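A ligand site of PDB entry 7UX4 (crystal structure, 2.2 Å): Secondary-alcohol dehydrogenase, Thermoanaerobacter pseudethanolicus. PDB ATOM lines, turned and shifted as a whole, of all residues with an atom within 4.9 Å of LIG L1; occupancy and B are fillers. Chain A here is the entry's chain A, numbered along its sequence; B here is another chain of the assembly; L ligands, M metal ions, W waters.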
ATOM      1  N   CYS A  37     -19.013  -9.431 -19.917  1.00  0.00           N
ATOM      2  CA  CYS A  37     -19.783 -10.648 -20.146  1.00  0.00           C
ATOM      3  C   CYS A  37     -18.830 -11.778 -20.520  1.00  0.00           C
ATOM      4  O   CYS A  37     -17.673 -11.562 -20.876  1.00  0.00           O
ATOM      5  CB  CYS A  37     -20.832 -10.479 -21.251  1.00  0.00           C
ATOM      6  SG  CYS A  37     -21.828 -11.969 -21.565  1.00  0.00           S
ATOM      7  N   THR A  38     -19.357 -13.006 -20.438  1.00  0.00           N
ATOM      8  CA  THR A  38     -18.596 -14.161 -20.919  1.00  0.00           C
ATOM      9  C   THR A  38     -18.265 -14.009 -22.400  1.00  0.00           C
ATOM     10  O   THR A  38     -17.232 -14.521 -22.854  1.00  0.00           O
ATOM     11  CB  THR A  38     -19.384 -15.444 -20.671  1.00  0.00           C
ATOM     12  OG1 THR A  38     -20.706 -15.309 -21.198  1.00  0.00           O
ATOM     13  CG2 THR A  38     -19.457 -15.757 -19.193  1.00  0.00           C
ATOM     14  N   SER A  39     -19.119 -13.325 -23.152  1.00  0.00           N
ATOM     15  CA  SER A  39     -18.859 -13.108 -24.567  1.00  0.00           C
ATOM     16  C   SER A  39     -17.585 -12.286 -24.766  1.00  0.00           C
ATOM     17  O   SER A  39     -16.810 -12.558 -25.705  1.00  0.00           O
ATOM     18  CB  SER A  39     -20.057 -12.406 -25.220  1.00  0.00           C
ATOM     19  OG  SER A  39     -21.222 -13.216 -25.099  1.00  0.00           O
ATOM     20  N   HIS A  42     -14.793 -14.834 -24.367  1.00  0.00           N
ATOM     21  CA  HIS A  42     -14.690 -15.727 -25.525  1.00  0.00           C
ATOM     22  C   HIS A  42     -14.085 -15.009 -26.717  1.00  0.00           C
ATOM     23  O   HIS A  42     -13.338 -15.600 -27.503  1.00  0.00           O
ATOM     24  CB  HIS A  42     -16.063 -16.288 -25.870  1.00  0.00           C
ATOM     25  CG  HIS A  42     -16.650 -17.151 -24.806  1.00  0.00           C
ATOM     26  ND1 HIS A  42     -18.000 -17.209 -24.554  1.00  0.00           N
ATOM     27  CD2 HIS A  42     -16.065 -17.980 -23.905  1.00  0.00           C
ATOM     28  CE1 HIS A  42     -18.233 -18.048 -23.549  1.00  0.00           C
ATOM     29  NE2 HIS A  42     -17.074 -18.517 -23.143  1.00  0.00           N
ATOM     30  N   ASP A 150     -28.204  -6.751 -21.967  1.00  0.00           N
ATOM     31  CA  ASP A 150     -27.861  -8.073 -22.494  1.00  0.00           C
ATOM     32  C   ASP A 150     -28.461  -9.202 -21.655  1.00  0.00           C
ATOM     33  O   ASP A 150     -29.175 -10.052 -22.187  1.00  0.00           O
ATOM     34  CB  ASP A 150     -26.350  -8.239 -22.576  1.00  0.00           C
ATOM     35  CG  ASP A 150     -25.943  -9.503 -23.331  1.00  0.00           C
ATOM     36  OD1 ASP A 150     -26.819 -10.137 -23.953  1.00  0.00           O
ATOM     37  OD2 ASP A 150     -24.750  -9.857 -23.298  1.00  0.00           O
ATOM     38  N   MET A 151     -28.154  -9.216 -20.355  1.00  0.00           N
ATOM     39  CA  MET A 151     -28.558 -10.341 -19.525  1.00  0.00           C
ATOM     40  C   MET A 151     -30.077 -10.495 -19.483  1.00  0.00           C
ATOM     41  O   MET A 151     -30.604 -11.596 -19.663  1.00  0.00           O
ATOM     42  CB  MET A 151     -27.989 -10.182 -18.114  1.00  0.00           C
ATOM     43  CG  MET A 151     -26.481 -10.046 -18.058  1.00  0.00           C
ATOM     44  SD  MET A 151     -25.588 -11.520 -18.595  1.00  0.00           S
ATOM     45  CE  MET A 151     -25.187 -11.123 -20.298  1.00  0.00           C
ATOM     46  N   THR A 154     -31.655 -11.323 -23.051  1.00  0.00           N
ATOM     47  CA  THR A 154     -31.323 -12.673 -23.503  1.00  0.00           C
ATOM     48  C   THR A 154     -32.152 -13.710 -22.742  1.00  0.00           C
ATOM     49  O   THR A 154     -32.847 -14.525 -23.349  1.00  0.00           O
ATOM     50  CB  THR A 154     -29.833 -12.960 -23.303  1.00  0.00           C
ATOM     51  OG1 THR A 154     -29.063 -11.992 -24.031  1.00  0.00           O
ATOM     52  CG2 THR A 154     -29.477 -14.350 -23.790  1.00  0.00           C
ATOM     53  N   GLY A 174     -28.762 -24.370 -16.806  1.00  0.00           N
ATOM     54  CA  GLY A 174     -27.741 -23.364 -16.620  1.00  0.00           C
ATOM     55  C   GLY A 174     -28.281 -22.139 -15.918  1.00  0.00           C
ATOM     56  O   GLY A 174     -29.202 -21.480 -16.416  1.00  0.00           O
ATOM     57  N   ILE A 175     -27.729 -21.818 -14.744  1.00  0.00           N
ATOM     58  CA  ILE A 175     -28.227 -20.683 -13.962  1.00  0.00           C
ATOM     59  C   ILE A 175     -27.115 -19.662 -13.784  1.00  0.00           C
ATOM     60  O   ILE A 175     -26.856 -19.197 -12.667  1.00  0.00           O
ATOM     61  CB  ILE A 175     -28.795 -21.146 -12.617  1.00  0.00           C
ATOM     62  CG1 ILE A 175     -27.797 -22.025 -11.864  1.00  0.00           C
ATOM     63  CG2 ILE A 175     -30.078 -21.905 -12.826  1.00  0.00           C
ATOM     64  CD1 ILE A 175     -28.247 -22.373 -10.464  1.00  0.00           C
ATOM     65  N   GLY A 176     -26.443 -19.313 -14.874  1.00  0.00           N
ATOM     66  CA  GLY A 176     -25.611 -18.135 -14.901  1.00  0.00           C
ATOM     67  C   GLY A 176     -26.505 -16.912 -14.995  1.00  0.00           C
ATOM     68  O   GLY A 176     -27.731 -17.004 -14.858  1.00  0.00           O
ATOM     69  N   PRO A 177     -25.912 -15.733 -15.212  1.00  0.00           N
ATOM     70  CA  PRO A 177     -26.736 -14.522 -15.310  1.00  0.00           C
ATOM     71  C   PRO A 177     -27.858 -14.633 -16.343  1.00  0.00           C
ATOM     72  O   PRO A 177     -28.995 -14.211 -16.080  1.00  0.00           O
ATOM     73  CB  PRO A 177     -25.718 -13.444 -15.684  1.00  0.00           C
ATOM     74  CG  PRO A 177     -24.423 -13.952 -15.168  1.00  0.00           C
ATOM     75  CD  PRO A 177     -24.471 -15.443 -15.319  1.00  0.00           C
ATOM     76  N   VAL A 178     -27.564 -15.206 -17.512  1.00  0.00           N
ATOM     77  CA  VAL A 178     -28.601 -15.394 -18.529  1.00  0.00           C
ATOM     78  C   VAL A 178     -29.644 -16.405 -18.033  1.00  0.00           C
ATOM     79  O   VAL A 178     -30.847 -16.171 -18.150  1.00  0.00           O
ATOM     80  CB  VAL A 178     -27.978 -15.853 -19.857  1.00  0.00           C
ATOM     81  CG1 VAL A 178     -29.048 -16.380 -20.798  1.00  0.00           C
ATOM     82  CG2 VAL A 178     -27.209 -14.712 -20.502  1.00  0.00           C
ATOM     83  N   GLY A 179     -29.189 -17.522 -17.476  1.00  0.00           N
ATOM     84  CA  GLY A 179     -30.122 -18.517 -16.975  1.00  0.00           C
ATOM     85  C   GLY A 179     -30.983 -17.984 -15.844  1.00  0.00           C
ATOM     86  O   GLY A 179     -32.178 -18.281 -15.773  1.00  0.00           O
ATOM     87  N   VAL A 197     -31.257 -25.872 -13.223  1.00  0.00           N
ATOM     88  CA  VAL A 197     -30.122 -26.790 -13.251  1.00  0.00           C
ATOM     89  C   VAL A 197     -28.844 -25.975 -13.135  1.00  0.00           C
ATOM     90  O   VAL A 197     -28.549 -25.133 -13.989  1.00  0.00           O
ATOM     91  CB  VAL A 197     -30.119 -27.642 -14.525  1.00  0.00           C
ATOM     92  CG1 VAL A 197     -28.945 -28.598 -14.505  1.00  0.00           C
ATOM     93  CG2 VAL A 197     -31.428 -28.390 -14.653  1.00  0.00           C
ATOM     94  N   GLY A 198     -28.074 -26.225 -12.075  1.00  0.00           N
ATOM     95  CA  GLY A 198     -26.856 -25.466 -11.853  1.00  0.00           C
ATOM     96  C   GLY A 198     -26.186 -25.933 -10.578  1.00  0.00           C
ATOM     97  O   GLY A 198     -26.687 -26.819  -9.867  1.00  0.00           O
ATOM     98  N   SER A 199     -25.033 -25.336 -10.291  1.00  0.00           N
ATOM     99  CA  SER A 199     -24.282 -25.842  -9.148  1.00  0.00           C
ATOM    100  C   SER A 199     -23.786 -24.764  -8.187  1.00  0.00           C
ATOM    101  O   SER A 199     -23.797 -25.004  -6.975  1.00  0.00           O
ATOM    102  CB  SER A 199     -23.093 -26.656  -9.652  1.00  0.00           C
ATOM    103  OG  SER A 199     -22.249 -25.872 -10.478  1.00  0.00           O
ATOM    104  N   ARG A 200     -23.364 -23.601  -8.681  1.00  0.00           N
ATOM    105  CA  ARG A 200     -22.723 -22.621  -7.794  1.00  0.00           C
ATOM    106  C   ARG A 200     -23.719 -22.082  -6.789  1.00  0.00           C
ATOM    107  O   ARG A 200     -24.816 -21.659  -7.166  1.00  0.00           O
ATOM    108  CB  ARG A 200     -22.079 -21.477  -8.596  1.00  0.00           C
ATOM    109  CG  ARG A 200     -20.828 -21.900  -9.347  1.00  0.00           C
ATOM    110  CD  ARG A 200     -19.986 -20.716  -9.802  1.00  0.00           C
ATOM    111  NE  ARG A 200     -20.683 -19.850 -10.749  1.00  0.00           N
ATOM    112  CZ  ARG A 200     -20.916 -18.562 -10.544  1.00  0.00           C
ATOM    113  NH1 ARG A 200     -20.520 -17.951  -9.436  1.00  0.00           N
ATOM    114  NH2 ARG A 200     -21.576 -17.871 -11.459  1.00  0.00           N
ATOM    115  N   CYS A 203     -25.427 -18.817  -7.326  1.00  0.00           N
ATOM    116  CA  CYS A 203     -26.390 -18.909  -8.409  1.00  0.00           C
ATOM    117  C   CYS A 203     -27.646 -19.657  -7.979  1.00  0.00           C
ATOM    118  O   CYS A 203     -28.755 -19.322  -8.415  1.00  0.00           O
ATOM    119  CB  CYS A 203     -25.754 -19.593  -9.614  1.00  0.00           C
ATOM    120  SG  CYS A 203     -24.392 -18.674 -10.358  1.00  0.00           S
ATOM    121  N   ILE A 223     -28.759 -35.276 -15.241  1.00  0.00           N
ATOM    122  CA  ILE A 223     -29.868 -34.323 -15.265  1.00  0.00           C
ATOM    123  C   ILE A 223     -31.132 -34.984 -15.781  1.00  0.00           C
ATOM    124  O   ILE A 223     -32.224 -34.783 -15.227  1.00  0.00           O
ATOM    125  CB  ILE A 223     -29.487 -33.100 -16.121  1.00  0.00           C
ATOM    126  CG1 ILE A 223     -28.298 -32.352 -15.535  1.00  0.00           C
ATOM    127  CG2 ILE A 223     -30.690 -32.181 -16.325  1.00  0.00           C
ATOM    128  CD1 ILE A 223     -27.741 -31.291 -16.463  1.00  0.00           C
ATOM    129  N   ALA A 242     -29.442 -22.329 -21.276  1.00  0.00           N
ATOM    130  CA  ALA A 242     -28.679 -21.122 -20.988  1.00  0.00           C
ATOM    131  C   ALA A 242     -27.230 -21.445 -20.615  1.00  0.00           C
ATOM    132  O   ALA A 242     -26.565 -20.600 -20.017  1.00  0.00           O
ATOM    133  CB  ALA A 242     -29.341 -20.311 -19.885  1.00  0.00           C
ATOM    134  N   GLY A 243     -26.752 -22.631 -20.949  1.00  0.00           N
ATOM    135  CA  GLY A 243     -25.380 -23.000 -20.644  1.00  0.00           C
ATOM    136  C   GLY A 243     -25.117 -24.447 -20.988  1.00  0.00           C
ATOM    137  O   GLY A 243     -26.023 -25.207 -21.331  1.00  0.00           O
ATOM    138  N   GLY A 244     -23.844 -24.813 -20.898  1.00  0.00           N
ATOM    139  CA  GLY A 244     -23.416 -26.182 -21.118  1.00  0.00           C
ATOM    140  C   GLY A 244     -22.708 -26.347 -22.453  1.00  0.00           C
ATOM    141  O   GLY A 244     -22.575 -25.416 -23.247  1.00  0.00           O
ATOM    142  N   ASN A 245     -22.247 -27.581 -22.685  1.00  0.00           N
ATOM    143  CA  ASN A 245     -21.571 -27.950 -23.918  1.00  0.00           C
ATOM    144  C   ASN A 245     -22.608 -28.345 -24.964  1.00  0.00           C
ATOM    145  O   ASN A 245     -23.811 -28.183 -24.767  1.00  0.00           O
ATOM    146  CB  ASN A 245     -20.587 -29.092 -23.657  1.00  0.00           C
ATOM    147  CG  ASN A 245     -19.515 -28.729 -22.665  1.00  0.00           C
ATOM    148  OD1 ASN A 245     -19.078 -27.579 -22.607  1.00  0.00           O
ATOM    149  ND2 ASN A 245     -19.108 -29.698 -21.860  1.00  0.00           N
ATOM    150  N   ILE A 248     -25.669 -30.664 -24.050  1.00  0.00           N
ATOM    151  CA  ILE A 248     -26.838 -30.192 -23.322  1.00  0.00           C
ATOM    152  C   ILE A 248     -28.053 -30.100 -24.234  1.00  0.00           C
ATOM    153  O   ILE A 248     -29.185 -30.104 -23.754  1.00  0.00           O
ATOM    154  CB  ILE A 248     -26.550 -28.836 -22.648  1.00  0.00           C
ATOM    155  CG1 ILE A 248     -27.488 -28.609 -21.459  1.00  0.00           C
ATOM    156  CG2 ILE A 248     -26.695 -27.699 -23.638  1.00  0.00           C
ATOM    157  CD1 ILE A 248     -27.322 -29.632 -20.364  1.00  0.00           C
ATOM    158  N   VAL A 265     -30.808 -20.060 -25.839  1.00  0.00           N
ATOM    159  CA  VAL A 265     -30.104 -18.790 -25.955  1.00  0.00           C
ATOM    160  C   VAL A 265     -28.623 -18.934 -25.658  1.00  0.00           C
ATOM    161  O   VAL A 265     -27.900 -17.934 -25.649  1.00  0.00           O
ATOM    162  CB  VAL A 265     -30.734 -17.699 -25.063  1.00  0.00           C
ATOM    163  CG1 VAL A 265     -32.109 -17.319 -25.601  1.00  0.00           C
ATOM    164  CG2 VAL A 265     -30.813 -18.171 -23.625  1.00  0.00           C
ATOM    165  N   ASN A 266     -28.159 -20.158 -25.407  1.00  0.00           N
ATOM    166  CA  ASN A 266     -26.756 -20.416 -25.129  1.00  0.00           C
ATOM    167  C   ASN A 266     -25.922 -20.229 -26.395  1.00  0.00           C
ATOM    168  O   ASN A 266     -26.408 -20.374 -27.518  1.00  0.00           O
ATOM    169  CB  ASN A 266     -26.597 -21.839 -24.580  1.00  0.00           C
ATOM    170  CG  ASN A 266     -25.166 -22.184 -24.223  1.00  0.00           C
ATOM    171  OD1 ASN A 266     -24.416 -21.342 -23.719  1.00  0.00           O
ATOM    172  ND2 ASN A 266     -24.778 -23.430 -24.475  1.00  0.00           N
ATOM    173  N   TYR A 267     -24.657 -19.876 -26.192  1.00  0.00           N
ATOM    174  CA  TYR A 267     -23.697 -19.718 -27.276  1.00  0.00           C
ATOM    175  C   TYR A 267     -22.763 -20.926 -27.288  1.00  0.00           C
ATOM    176  O   TYR A 267     -21.911 -21.074 -26.405  1.00  0.00           O
ATOM    177  CB  TYR A 267     -22.913 -18.412 -27.101  1.00  0.00           C
ATOM    178  CG  TYR A 267     -21.713 -18.252 -28.005  1.00  0.00           C
ATOM    179  CD1 TYR A 267     -21.755 -18.639 -29.330  1.00  0.00           C
ATOM    180  CD2 TYR A 267     -20.532 -17.695 -27.517  1.00  0.00           C
ATOM    181  CE1 TYR A 267     -20.650 -18.494 -30.155  1.00  0.00           C
ATOM    182  CE2 TYR A 267     -19.426 -17.538 -28.330  1.00  0.00           C
ATOM    183  CZ  TYR A 267     -19.493 -17.943 -29.651  1.00  0.00           C
ATOM    184  OH  TYR A 267     -18.387 -17.788 -30.454  1.00  0.00           O
ATOM    185  N   GLY A 293     -32.129 -18.344 -30.675  1.00  0.00           N
ATOM    186  CA  GLY A 293     -32.144 -16.985 -31.180  1.00  0.00           C
ATOM    187  C   GLY A 293     -31.203 -16.072 -30.436  1.00  0.00           C
ATOM    188  O   GLY A 293     -30.983 -16.198 -29.229  1.00  0.00           O
ATOM    189  N   LEU A 294     -30.637 -15.125 -31.180  1.00  0.00           N
ATOM    190  CA  LEU A 294     -29.905 -14.010 -30.596  1.00  0.00           C
ATOM    191  C   LEU A 294     -30.875 -13.093 -29.855  1.00  0.00           C
ATOM    192  O   LEU A 294     -32.050 -12.960 -30.213  1.00  0.00           O
ATOM    193  CB  LEU A 294     -29.185 -13.223 -31.691  1.00  0.00           C
ATOM    194  CG  LEU A 294     -28.175 -12.178 -31.254  1.00  0.00           C
ATOM    195  CD1 LEU A 294     -26.910 -12.872 -30.806  1.00  0.00           C
ATOM    196  CD2 LEU A 294     -27.873 -11.213 -32.391  1.00  0.00           C
ATOM    197  N   CYS A 295     -30.366 -12.444 -28.809  1.00  0.00           N
ATOM    198  CA  CYS A 295     -31.214 -11.610 -27.978  1.00  0.00           C
ATOM    199  C   CYS A 295     -31.730 -10.412 -28.772  1.00  0.00           C
ATOM    200  O   CYS A 295     -31.016  -9.865 -29.615  1.00  0.00           O
ATOM    201  CB  CYS A 295     -30.460 -11.118 -26.740  1.00  0.00           C
ATOM    202  SG  CYS A 295     -29.124  -9.953 -27.094  1.00  0.00           S
ATOM    203  N   LYS A 340     -13.439 -16.151 -12.701  1.00  0.00           N
ATOM    204  CA  LYS A 340     -14.720 -16.686 -12.255  1.00  0.00           C
ATOM    205  C   LYS A 340     -14.676 -17.193 -10.820  1.00  0.00           C
ATOM    206  O   LYS A 340     -14.606 -18.410 -10.590  1.00  0.00           O
ATOM    207  CB  LYS A 340     -15.177 -17.814 -13.180  1.00  0.00           C
ATOM    208  CG  LYS A 340     -16.612 -18.232 -12.994  1.00  0.00           C
ATOM    209  CD  LYS A 340     -16.921 -19.434 -13.865  1.00  0.00           C
ATOM    210  CE  LYS A 340     -16.229 -20.667 -13.304  1.00  0.00           C
ATOM    211  NZ  LYS A 340     -16.581 -21.928 -14.028  1.00  0.00           N
ATOM    212  N   MET B 285     -27.992 -19.247 -32.257  1.00  0.00           N
ATOM    213  CA  MET B 285     -28.674 -17.970 -32.154  1.00  0.00           C
ATOM    214  C   MET B 285     -29.129 -17.428 -33.514  1.00  0.00           C
ATOM    215  O   MET B 285     -29.306 -16.211 -33.653  1.00  0.00           O
ATOM    216  CB  MET B 285     -27.751 -16.943 -31.453  1.00  0.00           C
ATOM    217  CG  MET B 285     -27.382 -17.333 -30.012  1.00  0.00           C
ATOM    218  SD  MET B 285     -26.067 -16.353 -29.268  1.00  0.00           S
ATOM    219  CE  MET B 285     -24.708 -16.622 -30.398  1.00  0.00           C
HETATM  220  P1  LIG L   1     -22.247 -18.631 -17.412  1.00  0.00           P
HETATM  221  O1  LIG L   1     -21.204 -19.093 -18.368  1.00  0.00           O
HETATM  222  O2  LIG L   1     -21.736 -18.708 -16.011  1.00  0.00           O
HETATM  223  O3  LIG L   1     -23.593 -19.663 -17.556  1.00  0.00           O
HETATM  224  C1  LIG L   1     -23.322 -21.082 -17.649  1.00  0.00           C
HETATM  225  C2  LIG L   1     -24.299 -21.848 -16.731  1.00  0.00           C
HETATM  226  O4  LIG L   1     -24.431 -23.086 -17.151  1.00  0.00           O
HETATM  227  C3  LIG L   1     -23.664 -21.958 -15.343  1.00  0.00           C
HETATM  228  O5  LIG L   1     -24.612 -22.179 -14.392  1.00  0.00           O
HETATM  229  C4  LIG L   1     -22.800 -23.221 -15.526  1.00  0.00           C
HETATM  230  O6  LIG L   1     -22.336 -23.719 -14.178  1.00  0.00           O
HETATM  231  C5  LIG L   1     -23.675 -24.010 -16.075  1.00  0.00           C
HETATM  232  N1  LIG L   1     -23.043 -25.161 -16.754  1.00  0.00           N
HETATM  233  C6  LIG L   1     -21.823 -25.397 -17.280  1.00  0.00           C
HETATM  234  N2  LIG L   1     -21.835 -26.642 -17.769  1.00  0.00           N
HETATM  235  C7  LIG L   1     -23.050 -27.178 -17.550  1.00  0.00           C
HETATM  236  C8  LIG L   1     -23.603 -28.420 -17.842  1.00  0.00           C
HETATM  237  N3  LIG L   1     -23.039 -29.665 -18.535  1.00  0.00           N
HETATM  238  N4  LIG L   1     -24.833 -28.685 -17.503  1.00  0.00           N
HETATM  239  C9  LIG L   1     -25.602 -27.739 -16.857  1.00  0.00           C
HETATM  240  N5  LIG L   1     -25.063 -26.531 -16.563  1.00  0.00           N
HETATM  241  C10 LIG L   1     -23.795 -26.262 -16.918  1.00  0.00           C
HETATM  242  O7  LIG L   1     -22.668 -17.070 -17.770  1.00  0.00           O
HETATM  243  P2  LIG L   1     -23.915 -16.667 -18.812  1.00  0.00           P
HETATM  244  O8  LIG L   1     -23.742 -15.215 -19.289  1.00  0.00           O
HETATM  245  O9  LIG L   1     -25.284 -16.793 -18.073  1.00  0.00           O
HETATM  246  O10 LIG L   1     -23.865 -17.732 -20.090  1.00  0.00           O
HETATM  247  C11 LIG L   1     -24.987 -17.877 -20.924  1.00  0.00           C
HETATM  248  C12 LIG L   1     -24.516 -18.437 -22.307  1.00  0.00           C
HETATM  249  O11 LIG L   1     -25.205 -17.881 -23.281  1.00  0.00           O
HETATM  250  C13 LIG L   1     -23.045 -18.084 -22.563  1.00  0.00           C
HETATM  251  O12 LIG L   1     -22.445 -19.070 -23.265  1.00  0.00           O
HETATM  252  C14 LIG L   1     -23.119 -16.780 -23.391  1.00  0.00           C
HETATM  253  O13 LIG L   1     -21.909 -16.639 -24.288  1.00  0.00           O
HETATM  254  C15 LIG L   1     -24.212 -16.918 -24.108  1.00  0.00           C
HETATM  255  N6  LIG L   1     -24.891 -15.640 -24.332  1.00  0.00           N
HETATM  256  C16 LIG L   1     -25.816 -15.541 -25.345  1.00  0.00           C
HETATM  257  C17 LIG L   1     -26.486 -14.331 -25.570  1.00  0.00           C
HETATM  258  C18 LIG L   1     -27.538 -14.195 -26.722  1.00  0.00           C
HETATM  259  O14 LIG L   1     -27.765 -13.109 -27.219  1.00  0.00           O
HETATM  260  N7  LIG L   1     -28.257 -15.406 -27.241  1.00  0.00           N
HETATM  261  C19 LIG L   1     -26.218 -13.259 -24.778  1.00  0.00           C
HETATM  262  C20 LIG L   1     -25.293 -13.357 -23.765  1.00  0.00           C
HETATM  263  C21 LIG L   1     -24.630 -14.572 -23.552  1.00  0.00           C
HETATM  264  P3  LIG L   1     -21.185 -22.796 -13.410  1.00  0.00           P
HETATM  265  O15 LIG L   1     -20.209 -23.715 -12.658  1.00  0.00           O
HETATM  266  O16 LIG L   1     -21.859 -21.857 -12.418  1.00  0.00           O
HETATM  267  O17 LIG L   1     -20.423 -21.986 -14.435  1.00  0.00           O
HETATM  268  C1  LG2 L   2     -24.050 -11.103 -26.238  1.00  0.00           C
HETATM  269  C2  LG2 L   2     -23.383 -12.155 -27.140  1.00  0.00           C
HETATM  270  C3  LG2 L   2     -23.327 -11.733 -28.599  1.00  0.00           C
HETATM  271  C4  LG2 L   2     -23.163 -12.995 -29.472  1.00  0.00           C
HETATM  272  C5  LG2 L   2     -24.604 -10.979 -29.006  1.00  0.00           C
HETATM  273  C6  LG2 L   2     -24.819  -9.681 -28.224  1.00  0.00           C
HETATM  274  C7  LG2 L   2     -24.143  -9.700 -26.856  1.00  0.00           C
HETATM  275  O1  LG2 L   2     -23.316 -11.026 -25.029  1.00  0.00           O
HETATM  276 ZN    ZN M   1     -22.826  -9.833 -22.594  1.00  0.00          ZN
HETATM  277  O   HOH W   1     -21.607 -22.250 -23.830  1.00  0.00           O
HETATM  278  O   HOH W   2     -26.507 -18.997 -17.819  1.00  0.00           O
HETATM  279  O   HOH W   3     -24.004 -23.440 -11.554  1.00  0.00           O
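The backbone NH (N) of Ile 175 sits at hydrogen-bond distance from an oxygen (O5) of LIG L1 (3.2 Å).
OD1 of Asn 266 sits at hydrogen-bond distance from O12 of LIG L1 (3.0 Å).
The backbone carbonyl oxygen of Val 265 sits at hydrogen-bond distance from a nitrogen (N7) of LIG L1, at 3.0 Å.
An oxygen (O17) of LIG L1 lies within salt-bridge range of the side-chain amino group (NZ) of Lys 340, 3.9 Å away.
The side-chain hydroxyl of Ser 39 lies within hydrogen-bond range of an oxygen (O1) of LG2 L2.
N7 of LIG L1 lies within hydrogen-bond range of SD of Met 285 of chain B (3.1 Å).
O16 of LIG L1 lies within salt-bridge range of NE of Arg 200, 2.9 Å away.
O1 of LG2 L2 sits close to OD2 of Asp 150, 2.5 Å away.
N of Cys 295 lies within hydrogen-bond range of O14 of LIG L1.
An oxygen (O9) of LIG L1 is in hydrogen-bond range of the backbone NH of Val 178 (2.8 Å).
The backbone NH of Gly 176 is in hydrogen-bond range of an oxygen (O5) of LIG L1, at 3.4 Å.
The backbone carbonyl oxygen of Gly 293 lies within hydrogen-bond range of a nitrogen (N7) of LIG L1, at 3.5 Å.
An oxygen (O14) of LIG L1 sits close to the side-chain sulfur (SG) of Cys 295 (3.4 Å).
Water W2 lies within hydrogen-bond range of an oxygen (O9) of LIG L1, the backbone carbonyl oxygen of Ala 242, the backbone NH of Gly 176 and the backbone NH of Gly 179.
Water W3 lies within hydrogen-bond range of the backbone NH (N) of Ser 199 (2.5 Å), an oxygen (O16) of LIG L1 (2.8 Å) and the backbone NH (N) of Arg 200 (2.9 Å).
The backbone nitrogen of Pro 177 sits close to an oxygen (O9) of LIG L1 (3.1 Å).
Thr 38 touches LIG L1 (OG1 to O13, 3.6 Å).
Ser 39 touches LIG L1 (OG to O13, 3.6 Å).
His 42 touches LIG L1.
Asp 150 touches LIG L1.
OG1 of Thr 154 touches C19 of LIG L1 (3.2 Å).
CA of Gly 174 touches O4 of LIG L1, 3.4 Å away.
OG of Ser 199 touches O15 of LIG L1 (3.7 Å).
Ala 242 touches LIG L1.
Gly 243 touches LIG L1.
CA of Gly 244 touches C7 of LIG L1, at 3.7 Å.
Ile 248 touches LIG L1 (CD1 to N4, 3.9 Å).
Tyr 267 touches LIG L1.
Leu 294 touches LIG L1 (CD1 to O14, 3.7 Å).
Hydrophobic or aromatic side chains that line LIG L1: Pro 177, Val 178, Ile 248, Tyr 267, Leu 294 and Met 285 of chain B.
24 residues have an atom within 4 Å of LIG L1: Thr 38, Ser 39, His 42, Asp 150, Thr 154, Gly 174, Ile 175, Gly 176, Pro 177, Val 178, Ser 199, Arg 200, Ala 242, Gly 243, Gly 244, Ile 248, Val 265, Asn 266, Tyr 267, Gly 293, Leu 294, Cys 295, Lys 340 and Met 285 of chain B.
The side-chain hydroxyl (OG1) of Thr 154 lies close to the side-chain sulfur (SG) of Cys 295 (3.7 Å).
The backbone carbonyl oxygen (O) of Asp 150 sits at hydrogen-bond distance from the side-chain hydroxyl (OG1) of Thr 154, at 2.7 Å.
The side-chain sulfur of Cys 203 lies close to the backbone carbonyl oxygen of Ile 175 (3.4 Å).
The side-chain sulfur of Cys 203 sits at hydrogen-bond distance from the guanidinium group of Arg 200, 3.1 Å away.
The backbone NH of Leu 294 lies within hydrogen-bond range of the backbone carbonyl oxygen of Met 285 of chain B.
The side-chain hydroxyl of Thr 38 lies close to the side-chain sulfur of Cys 37, 3.5 Å away.
ND2 of Asn 266 is in hydrogen-bond range of O of Gly 244 (3.2 Å).
O of Val 197 is in hydrogen-bond range of N of Ile 175 (3.5 Å).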
